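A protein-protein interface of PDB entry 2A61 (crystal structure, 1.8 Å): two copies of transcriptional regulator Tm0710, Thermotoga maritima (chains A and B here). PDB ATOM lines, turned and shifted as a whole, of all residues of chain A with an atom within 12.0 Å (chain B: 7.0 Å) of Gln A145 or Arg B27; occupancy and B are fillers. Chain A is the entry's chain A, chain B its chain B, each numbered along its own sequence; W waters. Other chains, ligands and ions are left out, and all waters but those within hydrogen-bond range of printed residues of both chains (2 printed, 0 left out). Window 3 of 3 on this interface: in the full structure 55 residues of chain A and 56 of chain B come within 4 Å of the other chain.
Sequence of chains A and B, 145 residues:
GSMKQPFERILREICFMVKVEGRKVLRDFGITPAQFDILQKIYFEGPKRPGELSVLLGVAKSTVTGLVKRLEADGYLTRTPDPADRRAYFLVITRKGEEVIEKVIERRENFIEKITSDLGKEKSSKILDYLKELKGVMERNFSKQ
Water W2 lies within hydrogen-bond range of O of Asn A141 and OE2 of Glu B21. Water W1 bridges the chain-end carboxylate (O) of Gln A145 and the guanidinium group (NH1) of Arg B27.
Leu A56 touches none of the printed residues of chain B. Arg A140 touches none of the printed residues of chain B. Printed residues of chain B within 4 Å of Phe A142: Val B20, Glu B21 and Lys B24. Gln A145 touches two residues of chain B. Of the printed residues of chain A, Val B20 touches Phe A142 (3.6 Å). Lys B24 touches just these residues of chain A: Phe A142 and Lys A144. No residue of chain A comes within 4 Å of Val B25. No residue of chain A comes within 4 Å of Leu B26. Arg B27 touches just one residue of chain A: Gln A145. No residue of chain A comes within 4 Å of Gly B30. Printed residues of chain A within 4 Å of Arg B107: Lys A144 (3.6 Å) and Gln A145 (3.0 Å). The nearest residue of chain A that does not touch Arg B27 is Lys A144 (5.3 Å). The nearest printed residue of chain A that does not touch Val B20 is Lys A41 (6.8 Å).
Among the printed residues, pairs that only touch across the chains: Phe A142 with Val B20 (3.6 Å), Phe A142 with Glu B21 (3.8 Å) and Lys A144 with Arg B107 (3.6 Å).
NE2 of Gln A145 is in hydrogen-bond range of O of Ser A143. The side-chain carboxylate (OE1) of Glu B21 is in salt-bridge range of the side-chain amino group (NZ) of Lys B24 (3.0 Å). OE2 of Glu B21 is in salt-bridge range of NH1 of Arg B107 (2.7 Å).
Of the 12 printed residues of chain B, 5 touch a printed residue of chain A. Hydrophobic or aromatic side chains of chain B within 4 Å of the printed part of chain A: Val B20. Of the 12 printed residues of chain A, 3 touch a printed residue of chain B. Among the printed residues, 7 pairs touch across the chains. Among the printed residues, no Asp or Glu carboxylate lies within 4 Å of a Lys or Arg side-chain nitrogen of the other chain.
No position is printed for both chains.
NZ of Lys B24 is in hydrogen-bond range of O of Phe A142, 2.7 Å away. The backbone carbonyl oxygen (O) of Lys A144 sits at hydrogen-bond distance from the side-chain amino group (NZ) of Lys B24, at 2.7 Å. NH1 of Arg B27 lies within hydrogen-bond range of OE1 of Gln A145, at 2.8 Å. The chain-end carboxylate of Gln A145 is in salt-bridge range of the guanidinium group of Arg B107 (3.0 Å).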
ATOM      1  N   LYS A  41      29.067 -32.183   3.793  1.00  0.00           N
ATOM      2  CA  LYS A  41      28.627 -32.674   5.096  1.00  0.00           C
ATOM      3  C   LYS A  41      29.756 -33.303   5.908  1.00  0.00           C
ATOM      4  O   LYS A  41      29.909 -32.989   7.100  1.00  0.00           O
ATOM      5  CB  LYS A  41      27.489 -33.662   4.929  1.00  0.00           C
ATOM      6  CG  LYS A  41      26.937 -34.221   6.218  1.00  0.00           C
ATOM      7  CD  LYS A  41      26.514 -33.130   7.252  1.00  0.00           C
ATOM      8  CE  LYS A  41      25.417 -32.169   6.749  1.00  0.00           C
ATOM      9  NZ  LYS A  41      25.038 -31.036   7.719  1.00  0.00           N
ATOM     10  N   GLU A  45      31.222 -31.804   9.291  1.00  0.00           N
ATOM     11  CA  GLU A  45      30.833 -32.554  10.485  1.00  0.00           C
ATOM     12  C   GLU A  45      31.657 -33.802  10.749  1.00  0.00           C
ATOM     13  O   GLU A  45      31.523 -34.441  11.802  1.00  0.00           O
ATOM     14  CB  GLU A  45      29.356 -32.908  10.432  1.00  0.00           C
ATOM     15  CG  GLU A  45      28.484 -31.788   9.964  1.00  0.00           C
ATOM     16  CD  GLU A  45      27.037 -32.044  10.268  1.00  0.00           C
ATOM     17  OE1 GLU A  45      26.266 -31.065  10.275  1.00  0.00           O
ATOM     18  OE2 GLU A  45      26.673 -33.212  10.558  1.00  0.00           O
ATOM     19  N   VAL A  55      19.901 -40.509   5.154  1.00  0.00           N
ATOM     20  CA  VAL A  55      18.951 -39.640   5.873  1.00  0.00           C
ATOM     21  C   VAL A  55      19.177 -38.188   5.466  1.00  0.00           C
ATOM     22  O   VAL A  55      18.208 -37.481   5.214  1.00  0.00           O
ATOM     23  CB  VAL A  55      19.029 -39.843   7.421  1.00  0.00           C
ATOM     24  CG1 VAL A  55      18.204 -38.807   8.161  1.00  0.00           C
ATOM     25  CG2 VAL A  55      18.550 -41.278   7.804  1.00  0.00           C
ATOM     26  N   LEU A  56      20.443 -37.769   5.401  1.00  0.00           N
ATOM     27  CA  LEU A  56      20.830 -36.422   4.983  1.00  0.00           C
ATOM     28  C   LEU A  56      20.326 -36.043   3.600  1.00  0.00           C
ATOM     29  O   LEU A  56      19.710 -34.975   3.407  1.00  0.00           O
ATOM     30  CB  LEU A  56      22.378 -36.276   4.995  1.00  0.00           C
ATOM     31  CG  LEU A  56      22.979 -35.094   4.200  1.00  0.00           C
ATOM     32  CD1 LEU A  56      22.939 -33.736   5.003  1.00  0.00           C
ATOM     33  CD2 LEU A  56      24.377 -35.447   3.682  1.00  0.00           C
ATOM     34  N   MET A 138      20.203 -14.374  14.890  1.00  0.00           N
ATOM     35  CA  MET A 138      19.858 -15.718  14.412  1.00  0.00           C
ATOM     36  C   MET A 138      20.424 -16.796  15.319  1.00  0.00           C
ATOM     37  O   MET A 138      19.763 -17.768  15.609  1.00  0.00           O
ATOM     38  CB  MET A 138      20.343 -15.952  12.981  1.00  0.00           C
ATOM     39  CG  MET A 138      19.502 -15.248  11.941  1.00  0.00           C
ATOM     40  SD  MET A 138      20.061 -15.630  10.302  1.00  0.00           S
ATOM     41  CE  MET A 138      18.686 -14.952   9.344  1.00  0.00           C
ATOM     42  N   GLU A 139      21.678 -16.655  15.706  1.00  0.00           N
ATOM     43  CA  GLU A 139      22.315 -17.585  16.667  1.00  0.00           C
ATOM     44  C   GLU A 139      21.565 -17.759  17.991  1.00  0.00           C
ATOM     45  O   GLU A 139      21.487 -18.882  18.547  1.00  0.00           O
ATOM     46  CB  GLU A 139      23.739 -17.138  16.921  1.00  0.00           C
ATOM     47  CG  GLU A 139      24.647 -17.540  15.756  1.00  0.00           C
ATOM     48  CD  GLU A 139      26.021 -16.933  15.847  1.00  0.00           C
ATOM     49  OE1 GLU A 139      26.305 -16.135  16.795  1.00  0.00           O
ATOM     50  OE2 GLU A 139      26.811 -17.241  14.946  1.00  0.00           O
ATOM     51  N   ARG A 140      21.036 -16.647  18.485  1.00  0.00           N
ATOM     52  CA  ARG A 140      20.293 -16.567  19.727  1.00  0.00           C
ATOM     53  C   ARG A 140      18.977 -17.324  19.629  1.00  0.00           C
ATOM     54  O   ARG A 140      18.479 -17.808  20.644  1.00  0.00           O
ATOM     55  CB  ARG A 140      20.046 -15.090  20.079  1.00  0.00           C
ATOM     56  CG  ARG A 140      19.184 -14.866  21.338  1.00  0.00           C
ATOM     57  CD  ARG A 140      18.839 -13.388  21.534  1.00  0.00           C
ATOM     58  NE  ARG A 140      20.033 -12.558  21.341  1.00  0.00           N
ATOM     59  CZ  ARG A 140      20.006 -11.310  20.874  1.00  0.00           C
ATOM     60  NH1 ARG A 140      18.839 -10.743  20.556  1.00  0.00           N
ATOM     61  NH2 ARG A 140      21.143 -10.632  20.724  1.00  0.00           N
ATOM     62  N   ASN A 141      18.450 -17.489  18.405  1.00  0.00           N
ATOM     63  CA  ASN A 141      17.140 -18.132  18.155  1.00  0.00           C
ATOM     64  C   ASN A 141      17.152 -19.520  17.459  1.00  0.00           C
ATOM     65  O   ASN A 141      16.105 -20.182  17.281  1.00  0.00           O
ATOM     66  CB  ASN A 141      16.241 -17.142  17.382  1.00  0.00           C
ATOM     67  CG  ASN A 141      15.788 -15.938  18.250  1.00  0.00           C
ATOM     68  OD1 ASN A 141      16.336 -14.826  18.170  1.00  0.00           O
ATOM     69  ND2 ASN A 141      14.817 -16.183  19.107  1.00  0.00           N
ATOM     70  N   PHE A 142      18.342 -19.972  17.073  1.00  0.00           N
ATOM     71  CA  PHE A 142      18.501 -21.162  16.256  1.00  0.00           C
ATOM     72  C   PHE A 142      18.185 -22.471  16.988  1.00  0.00           C
ATOM     73  O   PHE A 142      18.041 -23.539  16.353  1.00  0.00           O
ATOM     74  CB  PHE A 142      19.929 -21.192  15.742  1.00  0.00           C
ATOM     75  CG  PHE A 142      20.149 -22.124  14.600  1.00  0.00           C
ATOM     76  CD1 PHE A 142      19.331 -22.071  13.456  1.00  0.00           C
ATOM     77  CD2 PHE A 142      21.220 -23.030  14.642  1.00  0.00           C
ATOM     78  CE1 PHE A 142      19.569 -22.946  12.364  1.00  0.00           C
ATOM     79  CE2 PHE A 142      21.482 -23.865  13.556  1.00  0.00           C
ATOM     80  CZ  PHE A 142      20.648 -23.832  12.417  1.00  0.00           C
ATOM     81  N   SER A 143      18.067 -22.399  18.319  1.00  0.00           N
ATOM     82  CA  SER A 143      17.768 -23.629  19.104  1.00  0.00           C
ATOM     83  C   SER A 143      16.272 -24.031  19.127  1.00  0.00           C
ATOM     84  O   SER A 143      15.922 -25.150  19.533  1.00  0.00           O
ATOM     85  CB  SER A 143      18.306 -23.493  20.558  1.00  0.00           C
ATOM     86  OG  SER A 143      17.512 -22.555  21.307  1.00  0.00           O
ATOM     87  N   LYS A 144      15.393 -23.144  18.666  1.00  0.00           N
ATOM     88  CA  LYS A 144      13.937 -23.389  18.754  1.00  0.00           C
ATOM     89  C   LYS A 144      13.513 -24.560  17.875  1.00  0.00           C
ATOM     90  O   LYS A 144      13.904 -24.652  16.704  1.00  0.00           O
ATOM     91  CB  LYS A 144      13.147 -22.124  18.400  1.00  0.00           C
ATOM     92  CG  LYS A 144      11.631 -22.235  18.678  1.00  0.00           C
ATOM     93  CD  LYS A 144      10.988 -20.847  18.648  1.00  0.00           C
ATOM     94  CE  LYS A 144       9.533 -20.886  18.219  1.00  0.00           C
ATOM     95  NZ  LYS A 144       9.015 -19.475  18.202  1.00  0.00           N
ATOM     96  N   GLN A 145      12.726 -25.466  18.455  1.00  0.00           N
ATOM     97  CA  GLN A 145      12.273 -26.635  17.757  1.00  0.00           C
ATOM     98  C   GLN A 145      10.927 -26.430  17.081  1.00  0.00           C
ATOM     99  O   GLN A 145      10.381 -27.423  16.574  1.00  0.00           O
ATOM    100  CB  GLN A 145      12.261 -27.850  18.693  1.00  0.00           C
ATOM    101  CG  GLN A 145      13.651 -28.134  19.298  1.00  0.00           C
ATOM    102  CD  GLN A 145      14.689 -28.420  18.213  1.00  0.00           C
ATOM    103  OE1 GLN A 145      14.652 -29.465  17.569  1.00  0.00           O
ATOM    104  NE2 GLN A 145      15.610 -27.500  18.016  1.00  0.00           N
ATOM    105  OXT GLN A 145      10.403 -25.301  16.977  1.00  0.00           O
ATOM    106  N   VAL B  20      18.271 -24.147   7.445  1.00  0.00           N
ATOM    107  CA  VAL B  20      17.954 -25.218   8.404  1.00  0.00           C
ATOM    108  C   VAL B  20      16.703 -24.887   9.196  1.00  0.00           C
ATOM    109  O   VAL B  20      15.884 -25.762   9.488  1.00  0.00           O
ATOM    110  CB  VAL B  20      19.170 -25.505   9.348  1.00  0.00           C
ATOM    111  CG1 VAL B  20      18.742 -26.327  10.583  1.00  0.00           C
ATOM    112  CG2 VAL B  20      20.302 -26.207   8.530  1.00  0.00           C
ATOM    113  N   GLU B  21      16.557 -23.617   9.551  1.00  0.00           N
ATOM    114  CA  GLU B  21      15.384 -23.171  10.309  1.00  0.00           C
ATOM    115  C   GLU B  21      14.074 -23.520   9.558  1.00  0.00           C
ATOM    116  O   GLU B  21      13.134 -24.120  10.139  1.00  0.00           O
ATOM    117  CB  GLU B  21      15.489 -21.667  10.570  1.00  0.00           C
ATOM    118  CG  GLU B  21      14.372 -21.110  11.464  1.00  0.00           C
ATOM    119  CD  GLU B  21      14.455 -21.705  12.851  1.00  0.00           C
ATOM    120  OE1 GLU B  21      15.586 -22.030  13.250  1.00  0.00           O
ATOM    121  OE2 GLU B  21      13.420 -21.865  13.519  1.00  0.00           O
ATOM    122  N   ARG B  23      13.595 -25.678   7.168  1.00  0.00           N
ATOM    123  CA  ARG B  23      13.479 -27.111   6.999  1.00  0.00           C
ATOM    124  C   ARG B  23      13.105 -27.875   8.277  1.00  0.00           C
ATOM    125  O   ARG B  23      12.802 -29.075   8.201  1.00  0.00           O
ATOM    126  CB  ARG B  23      14.760 -27.683   6.345  1.00  0.00           C
ATOM    127  CG  ARG B  23      14.905 -27.257   4.848  1.00  0.00           C
ATOM    128  CD  ARG B  23      16.216 -27.688   4.253  1.00  0.00           C
ATOM    129  NE  ARG B  23      16.280 -27.402   2.800  1.00  0.00           N
ATOM    130  CZ  ARG B  23      16.381 -28.309   1.828  1.00  0.00           C
ATOM    131  NH1 ARG B  23      16.415 -29.624   2.098  1.00  0.00           N
ATOM    132  NH2 ARG B  23      16.458 -27.890   0.556  1.00  0.00           N
ATOM    133  N   LYS B  24      13.065 -27.191   9.432  1.00  0.00           N
ATOM    134  CA  LYS B  24      12.599 -27.859  10.614  1.00  0.00           C
ATOM    135  C   LYS B  24      11.144 -28.277  10.446  1.00  0.00           C
ATOM    136  O   LYS B  24      10.703 -29.213  11.082  1.00  0.00           O
ATOM    137  CB  LYS B  24      12.742 -26.977  11.847  1.00  0.00           C
ATOM    138  CG  LYS B  24      14.177 -26.816  12.338  1.00  0.00           C
ATOM    139  CD  LYS B  24      14.305 -25.799  13.497  1.00  0.00           C
ATOM    140  CE  LYS B  24      15.807 -25.575  13.848  1.00  0.00           C
ATOM    141  NZ  LYS B  24      15.925 -24.471  14.893  1.00  0.00           N
ATOM    142  N   VAL B  25      10.385 -27.564   9.603  1.00  0.00           N
ATOM    143  CA  VAL B  25       8.950 -27.912   9.385  1.00  0.00           C
ATOM    144  C   VAL B  25       8.750 -29.269   8.694  1.00  0.00           C
ATOM    145  O   VAL B  25       7.712 -29.888   8.831  1.00  0.00           O
ATOM    146  CB  VAL B  25       8.087 -26.782   8.689  1.00  0.00           C
ATOM    147  CG1 VAL B  25       8.363 -25.374   9.280  1.00  0.00           C
ATOM    148  CG2 VAL B  25       8.315 -26.737   7.299  1.00  0.00           C
ATOM    149  N   LEU B  26       9.753 -29.726   7.967  1.00  0.00           N
ATOM    150  CA  LEU B  26       9.699 -31.021   7.281  1.00  0.00           C
ATOM    151  C   LEU B  26       9.660 -32.208   8.255  1.00  0.00           C
ATOM    152  O   LEU B  26       9.363 -33.319   7.865  1.00  0.00           O
ATOM    153  CB  LEU B  26      10.865 -31.160   6.293  1.00  0.00           C
ATOM    154  CG  LEU B  26      11.063 -30.013   5.315  1.00  0.00           C
ATOM    155  CD1 LEU B  26      12.304 -30.256   4.494  1.00  0.00           C
ATOM    156  CD2 LEU B  26       9.828 -29.812   4.391  1.00  0.00           C
ATOM    157  N   ARG B  27       9.940 -31.956   9.527  1.00  0.00           N
ATOM    158  CA  ARG B  27       9.832 -32.992  10.563  1.00  0.00           C
ATOM    159  C   ARG B  27       8.374 -33.433  10.708  1.00  0.00           C
ATOM    160  O   ARG B  27       8.111 -34.573  11.071  1.00  0.00           O
ATOM    161  CB  ARG B  27      10.393 -32.472  11.904  1.00  0.00           C
ATOM    162  CG  ARG B  27      11.906 -32.183  11.877  1.00  0.00           C
ATOM    163  CD  ARG B  27      12.359 -31.433  13.150  1.00  0.00           C
ATOM    164  NE  ARG B  27      13.790 -31.099  13.153  1.00  0.00           N
ATOM    165  CZ  ARG B  27      14.376 -30.282  14.042  1.00  0.00           C
ATOM    166  NH1 ARG B  27      13.667 -29.689  14.991  1.00  0.00           N
ATOM    167  NH2 ARG B  27      15.688 -30.057  13.979  1.00  0.00           N
ATOM    168  N   ASP B  28       7.435 -32.540  10.382  1.00  0.00           N
ATOM    169  CA  ASP B  28       5.987 -32.814  10.507  1.00  0.00           C
ATOM    170  C   ASP B  28       5.385 -33.454   9.246  1.00  0.00           C
ATOM    171  O   ASP B  28       4.249 -33.940   9.257  1.00  0.00           O
ATOM    172  CB  ASP B  28       5.251 -31.500  10.753  1.00  0.00           C
ATOM    173  CG  ASP B  28       5.597 -30.861  12.114  1.00  0.00           C
ATOM    174  OD1 ASP B  28       5.925 -31.577  13.084  1.00  0.00           O
ATOM    175  OD2 ASP B  28       5.514 -29.623  12.192  1.00  0.00           O
ATOM    176  N   PHE B  29       6.133 -33.427   8.153  1.00  0.00           N
ATOM    177  CA  PHE B  29       5.595 -33.856   6.861  1.00  0.00           C
ATOM    178  C   PHE B  29       6.080 -35.224   6.430  1.00  0.00           C
ATOM    179  O   PHE B  29       5.372 -35.933   5.695  1.00  0.00           O
ATOM    180  CB  PHE B  29       5.943 -32.837   5.802  1.00  0.00           C
ATOM    181  CG  PHE B  29       5.065 -31.649   5.804  1.00  0.00           C
ATOM    182  CD1 PHE B  29       5.499 -30.458   6.353  1.00  0.00           C
ATOM    183  CD2 PHE B  29       3.786 -31.713   5.228  1.00  0.00           C
ATOM    184  CE1 PHE B  29       4.674 -29.328   6.350  1.00  0.00           C
ATOM    185  CE2 PHE B  29       2.952 -30.600   5.197  1.00  0.00           C
ATOM    186  CZ  PHE B  29       3.387 -29.395   5.767  1.00  0.00           C
ATOM    187  N   GLY B  30       7.304 -35.572   6.830  1.00  0.00           N
ATOM    188  CA  GLY B  30       7.916 -36.815   6.461  1.00  0.00           C
ATOM    189  C   GLY B  30       8.373 -36.823   5.006  1.00  0.00           C
ATOM    190  O   GLY B  30       8.632 -37.883   4.461  1.00  0.00           O
ATOM    191  N   ILE B  31       8.459 -35.631   4.402  1.00  0.00           N
ATOM    192  CA  ILE B  31       9.089 -35.389   3.115  1.00  0.00           C
ATOM    193  C   ILE B  31      10.601 -35.312   3.347  1.00  0.00           C
ATOM    194  O   ILE B  31      11.051 -34.593   4.244  1.00  0.00           O
ATOM    195  CB  ILE B  31       8.609 -34.032   2.570  1.00  0.00           C
ATOM    196  CG1 ILE B  31       7.151 -34.132   2.142  1.00  0.00           C
ATOM    197  CG2 ILE B  31       9.466 -33.533   1.415  1.00  0.00           C
ATOM    198  CD1 ILE B  31       6.575 -32.786   1.818  1.00  0.00           C
ATOM    199  N   ARG B 107       7.910 -20.363   8.283  1.00  0.00           N
ATOM    200  CA  ARG B 107       8.867 -20.588   9.364  1.00  0.00           C
ATOM    201  C   ARG B 107      10.108 -19.714   9.203  1.00  0.00           C
ATOM    202  O   ARG B 107      10.578 -19.138  10.170  1.00  0.00           O
ATOM    203  CB  ARG B 107       9.199 -22.074   9.527  1.00  0.00           C
ATOM    204  CG  ARG B 107      10.492 -22.392  10.322  1.00  0.00           C
ATOM    205  CD  ARG B 107      10.446 -22.212  11.843  1.00  0.00           C
ATOM    206  NE  ARG B 107       9.997 -23.431  12.491  1.00  0.00           N
ATOM    207  CZ  ARG B 107      10.406 -23.932  13.660  1.00  0.00           C
ATOM    208  NH1 ARG B 107      11.374 -23.396  14.416  1.00  0.00           N
ATOM    209  NH2 ARG B 107       9.836 -25.049  14.053  1.00  0.00           N
HETATM  210  O   HOH W   1      10.477 -30.092  16.220  1.00  0.00           O
HETATM  211  O   HOH W   2      13.989 -20.160  15.779  1.00  0.00           O
